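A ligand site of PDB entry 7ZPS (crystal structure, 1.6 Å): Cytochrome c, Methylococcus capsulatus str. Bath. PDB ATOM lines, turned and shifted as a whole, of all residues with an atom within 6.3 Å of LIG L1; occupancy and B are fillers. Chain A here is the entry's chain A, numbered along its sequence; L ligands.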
ATOM      1  N   LYS A  38       0.307   2.456  18.757  1.00  0.00           N
ATOM      2  CA  LYS A  38      -0.810   1.588  18.300  1.00  0.00           C
ATOM      3  C   LYS A  38      -0.618   0.206  18.920  1.00  0.00           C
ATOM      4  O   LYS A  38       0.472  -0.061  19.485  1.00  0.00           O
ATOM      5  CB  LYS A  38      -0.786   1.473  16.782  1.00  0.00           C
ATOM      6  CG  LYS A  38       0.351   0.687  16.177  1.00  0.00           C
ATOM      7  CD  LYS A  38       0.249   0.398  14.730  1.00  0.00           C
ATOM      8  CE  LYS A  38      -0.903  -0.537  14.401  1.00  0.00           C
ATOM      9  NZ  LYS A  38      -0.856  -0.911  12.991  1.00  0.00           N
ATOM     10  N   SER A  39      -1.603  -0.659  18.748  1.00  0.00           N
ATOM     11  CA  SER A  39      -1.536  -2.066  19.181  1.00  0.00           C
ATOM     12  C   SER A  39      -2.181  -2.906  18.113  1.00  0.00           C
ATOM     13  O   SER A  39      -2.908  -2.373  17.246  1.00  0.00           O
ATOM     14  CB  SER A  39      -2.213  -2.272  20.468  1.00  0.00           C
ATOM     15  OG  SER A  39      -1.650  -1.389  21.456  1.00  0.00           O
ATOM     16  N   MET A  40      -1.945  -4.202  18.212  1.00  0.00           N
ATOM     17  CA  MET A  40      -2.574  -5.189  17.291  1.00  0.00           C
ATOM     18  C   MET A  40      -2.525  -6.528  18.030  1.00  0.00           C
ATOM     19  O   MET A  40      -1.591  -6.746  18.847  1.00  0.00           O
ATOM     20  CB  MET A  40      -1.785  -5.284  15.989  1.00  0.00           C
ATOM     21  CG  MET A  40      -2.432  -6.131  14.889  1.00  0.00           C
ATOM     22  SD  MET A  40      -1.414  -6.264  13.465  1.00  0.00           S
ATOM     23  CE  MET A  40      -1.612  -4.604  12.793  1.00  0.00           C
ATOM     24  N   ILE A  42      -2.131 -10.645  17.110  1.00  0.00           N
ATOM     25  CA  ILE A  42      -1.805 -11.634  16.068  1.00  0.00           C
ATOM     26  C   ILE A  42      -2.146 -12.993  16.703  1.00  0.00           C
ATOM     27  O   ILE A  42      -1.505 -13.363  17.704  1.00  0.00           O
ATOM     28  CB  ILE A  42      -0.362 -11.516  15.569  1.00  0.00           C
ATOM     29  CG1 ILE A  42      -0.168 -10.182  14.827  1.00  0.00           C
ATOM     30  CG2 ILE A  42       0.077 -12.732  14.750  1.00  0.00           C
ATOM     31  CD1 ILE A  42       1.180  -9.941  14.260  1.00  0.00           C
ATOM     32  N   LEU A  48       2.099 -14.260  10.602  1.00  0.00           N
ATOM     33  CA  LEU A  48       3.172 -13.735  11.472  1.00  0.00           C
ATOM     34  C   LEU A  48       3.140 -14.417  12.865  1.00  0.00           C
ATOM     35  O   LEU A  48       4.013 -14.061  13.710  1.00  0.00           O
ATOM     36  CB  LEU A  48       2.998 -12.214  11.592  1.00  0.00           C
ATOM     37  CG  LEU A  48       3.200 -11.398  10.298  1.00  0.00           C
ATOM     38  CD1 LEU A  48       3.129  -9.905  10.605  1.00  0.00           C
ATOM     39  CD2 LEU A  48       4.522 -11.722   9.617  1.00  0.00           C
ATOM     40  N   PHE A  52       5.726 -13.687  15.948  1.00  0.00           N
ATOM     41  CA  PHE A  52       5.174 -12.411  16.483  1.00  0.00           C
ATOM     42  C   PHE A  52       3.750 -12.576  16.986  1.00  0.00           C
ATOM     43  O   PHE A  52       3.104 -11.548  17.296  1.00  0.00           O
ATOM     44  CB  PHE A  52       5.344 -11.248  15.495  1.00  0.00           C
ATOM     45  CG  PHE A  52       6.751 -10.957  15.054  1.00  0.00           C
ATOM     46  CD1 PHE A  52       7.726 -10.557  15.966  1.00  0.00           C
ATOM     47  CD2 PHE A  52       7.107 -11.046  13.720  1.00  0.00           C
ATOM     48  CE1 PHE A  52       9.028 -10.280  15.545  1.00  0.00           C
ATOM     49  CE2 PHE A  52       8.394 -10.765  13.309  1.00  0.00           C
ATOM     50  CZ  PHE A  52       9.356 -10.380  14.207  1.00  0.00           C
ATOM     51  N   HIS A  56       0.672  -7.023  20.693  1.00  0.00           N
ATOM     52  CA  HIS A  56       1.843  -6.115  20.673  1.00  0.00           C
ATOM     53  C   HIS A  56       1.407  -4.657  20.680  1.00  0.00           C
ATOM     54  O   HIS A  56       0.310  -4.312  20.240  1.00  0.00           O
ATOM     55  CB  HIS A  56       2.772  -6.392  19.511  1.00  0.00           C
ATOM     56  CG  HIS A  56       2.281  -5.974  18.174  1.00  0.00           C
ATOM     57  ND1 HIS A  56       1.801  -6.914  17.294  1.00  0.00           N
ATOM     58  CD2 HIS A  56       2.282  -4.790  17.522  1.00  0.00           C
ATOM     59  CE1 HIS A  56       1.516  -6.315  16.137  1.00  0.00           C
ATOM     60  NE2 HIS A  56       1.780  -4.993  16.265  1.00  0.00           N
ATOM     61  N   VAL A  58       3.243  -0.780  20.077  1.00  0.00           N
ATOM     62  CA  VAL A  58       4.320  -0.011  19.463  1.00  0.00           C
ATOM     63  C   VAL A  58       4.504   1.305  20.216  1.00  0.00           C
ATOM     64  O   VAL A  58       3.538   1.948  20.574  1.00  0.00           O
ATOM     65  CB  VAL A  58       4.049   0.271  17.975  1.00  0.00           C
ATOM     66  CG1 VAL A  58       5.182   1.046  17.336  1.00  0.00           C
ATOM     67  CG2 VAL A  58       3.772  -1.029  17.218  1.00  0.00           C
ATOM     68  N   TYR A  59       5.756   1.540  20.599  1.00  0.00           N
ATOM     69  CA  TYR A  59       6.192   2.761  21.303  1.00  0.00           C
ATOM     70  C   TYR A  59       7.209   3.494  20.464  1.00  0.00           C
ATOM     71  O   TYR A  59       7.975   2.939  19.678  1.00  0.00           O
ATOM     72  CB  TYR A  59       6.810   2.448  22.669  1.00  0.00           C
ATOM     73  CG  TYR A  59       5.880   1.758  23.614  1.00  0.00           C
ATOM     74  CD1 TYR A  59       4.976   2.462  24.406  1.00  0.00           C
ATOM     75  CD2 TYR A  59       5.803   0.370  23.652  1.00  0.00           C
ATOM     76  CE1 TYR A  59       4.086   1.868  25.260  1.00  0.00           C
ATOM     77  CE2 TYR A  59       4.928  -0.242  24.524  1.00  0.00           C
ATOM     78  CZ  TYR A  59       4.039   0.461  25.296  1.00  0.00           C
ATOM     79  OH  TYR A  59       3.165  -0.094  26.158  1.00  0.00           O
ATOM     80  N   LEU A  79      11.928   3.015  17.722  1.00  0.00           N
ATOM     81  CA  LEU A  79      10.608   2.377  17.791  1.00  0.00           C
ATOM     82  C   LEU A  79      10.780   1.040  18.499  1.00  0.00           C
ATOM     83  O   LEU A  79      11.806   0.357  18.281  1.00  0.00           O
ATOM     84  CB  LEU A  79      10.114   2.160  16.368  1.00  0.00           C
ATOM     85  CG  LEU A  79       9.840   3.491  15.630  1.00  0.00           C
ATOM     86  CD1 LEU A  79       9.861   3.239  14.139  1.00  0.00           C
ATOM     87  CD2 LEU A  79       8.519   4.036  16.076  1.00  0.00           C
ATOM     88  N   VAL A  80       9.801   0.730  19.326  1.00  0.00           N
ATOM     89  CA  VAL A  80       9.795  -0.557  20.070  1.00  0.00           C
ATOM     90  C   VAL A  80       8.511  -1.312  19.773  1.00  0.00           C
ATOM     91  O   VAL A  80       7.415  -0.705  19.860  1.00  0.00           O
ATOM     92  CB  VAL A  80       9.960  -0.337  21.570  1.00  0.00           C
ATOM     93  CG1 VAL A  80       9.945  -1.664  22.337  1.00  0.00           C
ATOM     94  CG2 VAL A  80      11.194   0.463  21.861  1.00  0.00           C
ATOM     95  N   PHE A  81       8.651  -2.582  19.421  1.00  0.00           N
ATOM     96  CA  PHE A  81       7.555  -3.566  19.291  1.00  0.00           C
ATOM     97  C   PHE A  81       7.482  -4.420  20.547  1.00  0.00           C
ATOM     98  O   PHE A  81       8.446  -5.178  20.728  1.00  0.00           O
ATOM     99  CB  PHE A  81       7.856  -4.358  18.029  1.00  0.00           C
ATOM    100  CG  PHE A  81       6.862  -5.411  17.618  1.00  0.00           C
ATOM    101  CD1 PHE A  81       6.853  -6.668  18.225  1.00  0.00           C
ATOM    102  CD2 PHE A  81       5.965  -5.198  16.569  1.00  0.00           C
ATOM    103  CE1 PHE A  81       5.969  -7.661  17.794  1.00  0.00           C
ATOM    104  CE2 PHE A  81       5.093  -6.196  16.137  1.00  0.00           C
ATOM    105  CZ  PHE A  81       5.080  -7.426  16.769  1.00  0.00           C
ATOM    106  N   ILE A 101      10.815  -7.970  22.971  1.00  0.00           N
ATOM    107  CA  ILE A 101      10.692  -6.661  22.303  1.00  0.00           C
ATOM    108  C   ILE A 101      11.516  -6.691  21.025  1.00  0.00           C
ATOM    109  O   ILE A 101      12.588  -7.299  20.957  1.00  0.00           O
ATOM    110  CB  ILE A 101      11.001  -5.468  23.205  1.00  0.00           C
ATOM    111  CG1 ILE A 101      12.499  -5.324  23.499  1.00  0.00           C
ATOM    112  CG2 ILE A 101      10.160  -5.516  24.437  1.00  0.00           C
ATOM    113  CD1 ILE A 101      12.890  -4.099  24.272  1.00  0.00           C
ATOM    114  N   GLY A 102      10.990  -6.007  20.008  1.00  0.00           N
ATOM    115  CA  GLY A 102      11.763  -5.676  18.823  1.00  0.00           C
ATOM    116  C   GLY A 102      12.100  -4.179  18.866  1.00  0.00           C
ATOM    117  O   GLY A 102      11.295  -3.404  19.393  1.00  0.00           O
ATOM    118  N   VAL A 103      13.279  -3.849  18.395  1.00  0.00           N
ATOM    119  CA  VAL A 103      13.796  -2.471  18.501  1.00  0.00           C
ATOM    120  C   VAL A 103      14.362  -2.051  17.153  1.00  0.00           C
ATOM    121  O   VAL A 103      15.143  -2.811  16.535  1.00  0.00           O
ATOM    122  CB  VAL A 103      14.823  -2.334  19.634  1.00  0.00           C
ATOM    123  CG1 VAL A 103      15.313  -0.908  19.788  1.00  0.00           C
ATOM    124  CG2 VAL A 103      14.243  -2.841  20.945  1.00  0.00           C
ATOM    125  N   MET A 104      13.934  -0.869  16.682  1.00  0.00           N
ATOM    126  CA  MET A 104      14.566  -0.216  15.504  1.00  0.00           C
ATOM    127  C   MET A 104      15.190   1.108  15.986  1.00  0.00           C
ATOM    128  O   MET A 104      14.497   1.915  16.619  1.00  0.00           O
ATOM    129  CB  MET A 104      13.515   0.069  14.415  1.00  0.00           C
ATOM    130  CG  MET A 104      13.072  -1.151  13.680  1.00  0.00           C
ATOM    131  SD  MET A 104      11.554  -0.884  12.705  1.00  0.00           S
ATOM    132  CE  MET A 104      12.250   0.163  11.420  1.00  0.00           C
ATOM    133  N   GLY A 118      18.908   0.168  12.666  1.00  0.00           N
ATOM    134  CA  GLY A 118      19.478  -1.005  13.332  1.00  0.00           C
ATOM    135  C   GLY A 118      18.357  -1.842  13.910  1.00  0.00           C
ATOM    136  O   GLY A 118      17.502  -1.261  14.561  1.00  0.00           O
ATOM    137  N   TYR A 119      18.343  -3.151  13.671  1.00  0.00           N
ATOM    138  CA  TYR A 119      17.267  -4.049  14.119  1.00  0.00           C
ATOM    139  C   TYR A 119      17.826  -4.931  15.235  1.00  0.00           C
ATOM    140  O   TYR A 119      18.837  -5.594  14.988  1.00  0.00           O
ATOM    141  CB  TYR A 119      16.752  -4.871  12.941  1.00  0.00           C
ATOM    142  CG  TYR A 119      16.016  -4.064  11.900  1.00  0.00           C
ATOM    143  CD1 TYR A 119      16.685  -3.469  10.846  1.00  0.00           C
ATOM    144  CD2 TYR A 119      14.648  -3.967  11.976  1.00  0.00           C
ATOM    145  CE1 TYR A 119      15.989  -2.716   9.910  1.00  0.00           C
ATOM    146  CE2 TYR A 119      13.925  -3.296  11.002  1.00  0.00           C
ATOM    147  CZ  TYR A 119      14.613  -2.655   9.989  1.00  0.00           C
ATOM    148  OH  TYR A 119      13.921  -1.946   9.066  1.00  0.00           O
ATOM    149  N   GLU A 120      17.125  -5.011  16.349  1.00  0.00           N
ATOM    150  CA  GLU A 120      17.533  -5.944  17.444  1.00  0.00           C
ATOM    151  C   GLU A 120      16.298  -6.484  18.128  1.00  0.00           C
ATOM    152  O   GLU A 120      15.267  -5.793  18.205  1.00  0.00           O
ATOM    153  CB  GLU A 120      18.423  -5.232  18.447  1.00  0.00           C
ATOM    154  CG  GLU A 120      18.890  -6.115  19.596  1.00  0.00           C
ATOM    155  CD  GLU A 120      19.754  -7.301  19.203  1.00  0.00           C
ATOM    156  OE1 GLU A 120      19.199  -8.290  18.736  1.00  0.00           O
ATOM    157  OE2 GLU A 120      21.001  -7.172  19.322  1.00  0.00           O
ATOM    158  N   GLY A 121      16.379  -7.710  18.635  1.00  0.00           N
ATOM    159  CA  GLY A 121      15.347  -8.295  19.469  1.00  0.00           C
ATOM    160  C   GLY A 121      15.893  -8.598  20.852  1.00  0.00           C
ATOM    161  O   GLY A 121      17.103  -8.890  20.974  1.00  0.00           O
ATOM    162  N   LEU A 131      18.723 -11.209  20.402  1.00  0.00           N
ATOM    163  CA  LEU A 131      18.198 -12.293  19.553  1.00  0.00           C
ATOM    164  C   LEU A 131      18.783 -12.274  18.144  1.00  0.00           C
ATOM    165  O   LEU A 131      18.788 -13.299  17.530  1.00  0.00           O
ATOM    166  CB  LEU A 131      16.663 -12.193  19.505  1.00  0.00           C
ATOM    167  CG  LEU A 131      15.951 -12.300  20.837  1.00  0.00           C
ATOM    168  CD1 LEU A 131      14.462 -12.163  20.595  1.00  0.00           C
ATOM    169  CD2 LEU A 131      16.276 -13.621  21.499  1.00  0.00           C
ATOM    170  N   VAL A 132      19.139 -11.121  17.606  1.00  0.00           N
ATOM    171  CA  VAL A 132      19.454 -11.013  16.162  1.00  0.00           C
ATOM    172  C   VAL A 132      20.881 -11.503  15.948  1.00  0.00           C
ATOM    173  O   VAL A 132      21.758 -11.064  16.686  1.00  0.00           O
ATOM    174  CB  VAL A 132      19.227  -9.585  15.649  1.00  0.00           C
ATOM    175  CG1 VAL A 132      19.895  -9.344  14.318  1.00  0.00           C
ATOM    176  CG2 VAL A 132      17.732  -9.314  15.594  1.00  0.00           C
ATOM    177  N   GLY A 136      20.644  -8.046  11.349  1.00  0.00           N
ATOM    178  CA  GLY A 136      19.275  -7.526  11.094  1.00  0.00           C
ATOM    179  C   GLY A 136      18.877  -7.663   9.621  1.00  0.00           C
ATOM    180  O   GLY A 136      17.818  -7.117   9.262  1.00  0.00           O
ATOM    181  N   GLY A 138      17.529 -10.332   8.147  1.00  0.00           N
ATOM    182  CA  GLY A 138      16.208 -10.991   8.201  1.00  0.00           C
ATOM    183  C   GLY A 138      15.078 -10.003   8.508  1.00  0.00           C
ATOM    184  O   GLY A 138      14.018 -10.014   7.833  1.00  0.00           O
ATOM    185  N   CYS A 139      15.279  -9.145   9.504  1.00  0.00           N
ATOM    186  CA  CYS A 139      14.288  -8.134   9.907  1.00  0.00           C
ATOM    187  C   CYS A 139      14.089  -7.196   8.707  1.00  0.00           C
ATOM    188  O   CYS A 139      12.907  -6.911   8.352  1.00  0.00           O
ATOM    189  CB  CYS A 139      14.754  -7.301  11.093  1.00  0.00           C
ATOM    190  SG  CYS A 139      15.210  -8.246  12.557  1.00  0.00           S
ATOM    191  N   PHE A 140      15.198  -6.701   8.189  1.00  0.00           N
ATOM    192  CA  PHE A 140      15.240  -5.717   7.076  1.00  0.00           C
ATOM    193  C   PHE A 140      14.556  -6.320   5.854  1.00  0.00           C
ATOM    194  O   PHE A 140      13.842  -5.590   5.167  1.00  0.00           O
ATOM    195  CB  PHE A 140      16.674  -5.268   6.830  1.00  0.00           C
ATOM    196  CG  PHE A 140      16.812  -4.274   5.706  1.00  0.00           C
ATOM    197  CD1 PHE A 140      16.060  -3.114   5.716  1.00  0.00           C
ATOM    198  CD2 PHE A 140      17.724  -4.479   4.678  1.00  0.00           C
ATOM    199  CE1 PHE A 140      16.173  -2.199   4.678  1.00  0.00           C
ATOM    200  CE2 PHE A 140      17.841  -3.552   3.653  1.00  0.00           C
ATOM    201  CZ  PHE A 140      17.069  -2.424   3.666  1.00  0.00           C
ATOM    202  N   GLY A 141      14.714  -7.604   5.572  1.00  0.00           N
ATOM    203  CA  GLY A 141      14.086  -8.199   4.386  1.00  0.00           C
ATOM    204  C   GLY A 141      12.582  -8.006   4.388  1.00  0.00           C
ATOM    205  O   GLY A 141      12.008  -7.825   3.296  1.00  0.00           O
ATOM    206  N   CYS A 142      11.930  -8.060   5.541  1.00  0.00           N
ATOM    207  CA  CYS A 142      10.466  -7.844   5.651  1.00  0.00           C
ATOM    208  C   CYS A 142      10.164  -6.338   5.646  1.00  0.00           C
ATOM    209  O   CYS A 142       9.220  -5.866   4.936  1.00  0.00           O
ATOM    210  CB  CYS A 142       9.883  -8.526   6.868  1.00  0.00           C
ATOM    211  SG  CYS A 142       8.104  -8.478   6.914  1.00  0.00           S
ATOM    212  N   HIS A 143      10.850  -5.565   6.471  1.00  0.00           N
ATOM    213  CA  HIS A 143      10.579  -4.113   6.622  1.00  0.00           C
ATOM    214  C   HIS A 143      10.872  -3.371   5.281  1.00  0.00           C
ATOM    215  O   HIS A 143      10.320  -2.285   5.099  1.00  0.00           O
ATOM    216  CB  HIS A 143      11.318  -3.542   7.853  1.00  0.00           C
ATOM    217  CG  HIS A 143      10.623  -3.811   9.147  1.00  0.00           C
ATOM    218  ND1 HIS A 143       9.985  -2.816   9.849  1.00  0.00           N
ATOM    219  CD2 HIS A 143      10.457  -4.948   9.896  1.00  0.00           C
ATOM    220  CE1 HIS A 143       9.435  -3.345  10.944  1.00  0.00           C
ATOM    221  NE2 HIS A 143       9.676  -4.630  10.984  1.00  0.00           N
ATOM    222  N   TYR A 151      10.654   2.407   6.078  1.00  0.00           N
ATOM    223  CA  TYR A 151      10.816   1.006   6.591  1.00  0.00           C
ATOM    224  C   TYR A 151       9.989   0.807   7.847  1.00  0.00           C
ATOM    225  O   TYR A 151      10.124  -0.286   8.505  1.00  0.00           O
ATOM    226  CB  TYR A 151      12.284   0.708   6.823  1.00  0.00           C
ATOM    227  CG  TYR A 151      13.128   0.876   5.603  1.00  0.00           C
ATOM    228  CD1 TYR A 151      13.017  -0.024   4.555  1.00  0.00           C
ATOM    229  CD2 TYR A 151      13.976   1.960   5.457  1.00  0.00           C
ATOM    230  CE1 TYR A 151      13.791   0.102   3.414  1.00  0.00           C
ATOM    231  CE2 TYR A 151      14.754   2.099   4.319  1.00  0.00           C
ATOM    232  CZ  TYR A 151      14.661   1.168   3.307  1.00  0.00           C
ATOM    233  OH  TYR A 151      15.430   1.301   2.178  1.00  0.00           O
ATOM    234  N   VAL A 152       9.063   1.713   8.103  1.00  0.00           N
ATOM    235  CA  VAL A 152       8.140   1.652   9.265  1.00  0.00           C
ATOM    236  C   VAL A 152       6.737   1.276   8.814  1.00  0.00           C
ATOM    237  O   VAL A 152       6.180   1.940   7.913  1.00  0.00           O
ATOM    238  CB  VAL A 152       8.169   2.964  10.045  1.00  0.00           C
ATOM    239  CG1 VAL A 152       7.173   2.984  11.185  1.00  0.00           C
ATOM    240  CG2 VAL A 152       9.571   3.320  10.483  1.00  0.00           C
ATOM    241  N   PHE A 153       6.145   0.253   9.418  1.00  0.00           N
ATOM    242  CA  PHE A 153       4.770  -0.184   9.091  1.00  0.00           C
ATOM    243  C   PHE A 153       3.766   0.720   9.799  1.00  0.00           C
ATOM    244  O   PHE A 153       2.669   1.046   9.265  1.00  0.00           O
ATOM    245  CB  PHE A 153       4.507  -1.631   9.511  1.00  0.00           C
ATOM    246  CG  PHE A 153       5.188  -2.687   8.679  1.00  0.00           C
ATOM    247  CD1 PHE A 153       6.449  -3.152   8.997  1.00  0.00           C
ATOM    248  CD2 PHE A 153       4.561  -3.227   7.564  1.00  0.00           C
ATOM    249  CE1 PHE A 153       7.056  -4.166   8.258  1.00  0.00           C
ATOM    250  CE2 PHE A 153       5.162  -4.218   6.799  1.00  0.00           C
ATOM    251  CZ  PHE A 153       6.434  -4.693   7.146  1.00  0.00           C
ATOM    252  N   SER A 154       4.004   1.005  11.072  1.00  0.00           N
ATOM    253  CA  SER A 154       3.007   1.612  11.952  1.00  0.00           C
ATOM    254  C   SER A 154       2.669   3.014  11.446  1.00  0.00           C
ATOM    255  O   SER A 154       3.603   3.732  11.057  1.00  0.00           O
ATOM    256  CB  SER A 154       3.469   1.737  13.396  1.00  0.00           C
ATOM    257  OG  SER A 154       3.664   0.453  13.953  1.00  0.00           O
ATOM    258  N   ARG A 155       1.395   3.373  11.577  1.00  0.00           N
ATOM    259  CA  ARG A 155       0.920   4.741  11.279  1.00  0.00           C
ATOM    260  C   ARG A 155       0.421   5.369  12.557  1.00  0.00           C
ATOM    261  O   ARG A 155      -0.314   4.743  13.335  1.00  0.00           O
ATOM    262  CB  ARG A 155      -0.195   4.742  10.215  1.00  0.00           C
ATOM    263  CG  ARG A 155       0.202   4.086   8.903  1.00  0.00           C
ATOM    264  CD  ARG A 155       1.337   4.755   8.174  1.00  0.00           C
ATOM    265  NE  ARG A 155       1.611   3.952   6.979  1.00  0.00           N
ATOM    266  CZ  ARG A 155       2.770   3.348   6.684  1.00  0.00           C
ATOM    267  NH1 ARG A 155       3.849   3.498   7.436  1.00  0.00           N
ATOM    268  NH2 ARG A 155       2.834   2.593   5.604  1.00  0.00           N
HETATM  269 FE1  LIG L   1       8.864  -5.974  12.533  1.00  0.00          FE
HETATM  270  C1  LIG L   1       6.536  -3.592  13.306  1.00  0.00           C
HETATM  271  C2  LIG L   1      11.131  -4.521  14.704  1.00  0.00           C
HETATM  272  C3  LIG L   1      11.047  -8.413  11.871  1.00  0.00           C
HETATM  273  C4  LIG L   1       6.723  -7.237  10.172  1.00  0.00           C
HETATM  274  N1  LIG L   1       8.865  -4.378  13.750  1.00  0.00           N
HETATM  275  C5  LIG L   1       7.841  -3.488  13.905  1.00  0.00           C
HETATM  276  C6  LIG L   1       8.171  -2.355  14.829  1.00  0.00           C
HETATM  277  C7  LIG L   1       9.490  -2.660  15.201  1.00  0.00           C
HETATM  278  C8  LIG L   1       9.836  -3.862  14.530  1.00  0.00           C
HETATM  279  C9  LIG L   1      10.338  -1.848  16.147  1.00  0.00           C
HETATM  280  C10 LIG L   1       7.311  -1.197  15.126  1.00  0.00           C
HETATM  281  C11 LIG L   1       7.641  -0.162  13.983  1.00  0.00           C
HETATM  282  C12 LIG L   1       6.973  -0.395  12.605  1.00  0.00           C
HETATM  283  O1  LIG L   1       5.724  -0.399  12.672  1.00  0.00           O
HETATM  284  O2  LIG L   1       7.697  -0.628  11.599  1.00  0.00           O
HETATM  285  N2  LIG L   1      10.721  -6.422  13.186  1.00  0.00           N
HETATM  286  C13 LIG L   1      11.469  -5.740  14.060  1.00  0.00           C
HETATM  287  C14 LIG L   1      12.784  -6.427  14.331  1.00  0.00           C
HETATM  288  C15 LIG L   1      12.697  -7.619  13.538  1.00  0.00           C
HETATM  289  C16 LIG L   1      11.432  -7.461  12.838  1.00  0.00           C
HETATM  290  C17 LIG L   1      13.819  -5.937  15.326  1.00  0.00           C
HETATM  291  C18 LIG L   1      13.757  -8.719  13.348  1.00  0.00           C
HETATM  292  C19 LIG L   1      14.018  -9.286  14.733  1.00  0.00           C
HETATM  293  N3  LIG L   1       8.872  -7.549  11.269  1.00  0.00           N
HETATM  294  C20 LIG L   1       9.868  -8.416  11.097  1.00  0.00           C
HETATM  295  C21 LIG L   1       9.667  -9.404  10.015  1.00  0.00           C
HETATM  296  C22 LIG L   1       8.348  -9.006   9.538  1.00  0.00           C
HETATM  297  C23 LIG L   1       7.999  -7.870  10.339  1.00  0.00           C
HETATM  298  C24 LIG L   1      10.607 -10.482   9.627  1.00  0.00           C
HETATM  299  C25 LIG L   1       7.540  -9.502   8.346  1.00  0.00           C
HETATM  300  C26 LIG L   1       7.634 -10.996   8.184  1.00  0.00           C
HETATM  301  N4  LIG L   1       7.011  -5.481  11.879  1.00  0.00           N
HETATM  302  C27 LIG L   1       6.257  -6.160  10.964  1.00  0.00           C
HETATM  303  C28 LIG L   1       4.953  -5.650  10.814  1.00  0.00           C
HETATM  304  C29 LIG L   1       4.881  -4.581  11.756  1.00  0.00           C
HETATM  305  C30 LIG L   1       6.195  -4.585  12.366  1.00  0.00           C
HETATM  306  C31 LIG L   1       3.898  -6.111   9.864  1.00  0.00           C
HETATM  307  C32 LIG L   1       3.737  -3.627  12.025  1.00  0.00           C
HETATM  308  C33 LIG L   1       2.829  -4.189  13.128  1.00  0.00           C
HETATM  309  C34 LIG L   1       1.682  -3.316  13.493  1.00  0.00           C
HETATM  310  O3  LIG L   1       1.100  -3.221  14.577  1.00  0.00           O
HETATM  311  O4  LIG L   1       1.261  -2.526  12.504  1.00  0.00           O
HETATM  312  N1  LG2 L   2       8.114  -7.024  13.753  1.00  0.00           N
HETATM  313  O1  LG2 L   2       8.423  -6.976  14.978  1.00  0.00           O
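A nitrogen (N1) of LG2 L2 binds an iron atom (FE1) of LIG L1, 1.8 Å away.
O of Val 152 sits at hydrogen-bond distance from NH1 of Arg 155. The side-chain carboxylate (OE1) of Glu 120 lies within hydrogen-bond range of the backbone NH (N) of Leu 131. The side-chain carboxylate (OE1) of Glu 120 is in hydrogen-bond range of the backbone NH (N) of Val 132 (3.0 Å). The backbone carbonyl oxygen of Gly 102 is in hydrogen-bond range of the backbone NH of Phe 81 (2.8 Å). A ring nitrogen (ND1) of His 143 is in hydrogen-bond range of the backbone carbonyl oxygen (O) of Tyr 151, 2.9 Å away. A ring nitrogen (ND1) of His 143 sits close to the side-chain sulfur of Met 104, at 3.8 Å. The backbone NH of Met 104 sits at hydrogen-bond distance from the backbone carbonyl oxygen of Leu 79 (2.9 Å). The backbone NH (N) of Val 103 sits at hydrogen-bond distance from the backbone carbonyl oxygen (O) of Glu 120 (2.8 Å).
CE of Met 40 touches O3 of LIG L1, 3.5 Å away. Leu 48 touches LIG L1 (CD2 to C26, 3.5 Å). CZ of Phe 52 touches C3 of LIG L1, at 3.5 Å. Val 58 touches LIG L1 (CG1 to C10, 3.8 Å). O of Leu 79 touches C9 of LIG L1, at 3.4 Å. Phe 81 touches LIG L1 (CD2 to C5, 3.7 Å). Gly 102 touches LIG L1 (O to C9, 3.7 Å). O of Val 103 touches C17 of LIG L1, 3.6 Å away. Met 104 touches LIG L1 (SD to C7, 3.7 Å). Tyr 119 touches LIG L1. O of Glu 120 touches C17 of LIG L1 (3.2 Å). Val 132 touches LIG L1 (CG2 to C19, 3.8 Å). O of Gly 138 touches C24 of LIG L1 (3.9 Å). Tyr 151 touches LIG L1. Val 152 touches LIG L1. Hydrophobic or aromatic side chains that line LIG L1: Met 40, Leu 48, Phe 52, His 56, Val 58, Phe 81, Met 104, Tyr 119, Val 132, His 143, Val 152 and Phe 153. Of the 34 residues printed, 22 come within 4 Å of LIG L1.
OG of Ser 154 lies within hydrogen-bond range of O1 of LIG L1, 2.6 Å away. An oxygen (O2) of LIG L1 sits at hydrogen-bond distance from the backbone NH of Phe 153, 2.8 Å away. The backbone NH (N) of Ser 154 lies within hydrogen-bond range of an oxygen (O1) of LIG L1, 2.7 Å away. A ring nitrogen (NE2) of His 143 is bound to an iron atom (FE1) of LIG L1, 2.2 Å away. A carbon (C25) of LIG L1 is bonded to the side-chain sulfur (SG) of Cys 142, 1.8 Å away. C18 of LIG L1 is bonded to SG of Cys 139 (1.7 Å). The side-chain amino group (NZ) of Lys 38 is in salt-bridge range of an oxygen (O4) of LIG L1 (2.7 Å). NE2 of His 56 sits at hydrogen-bond distance from O3 of LIG L1 (2.5 Å).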
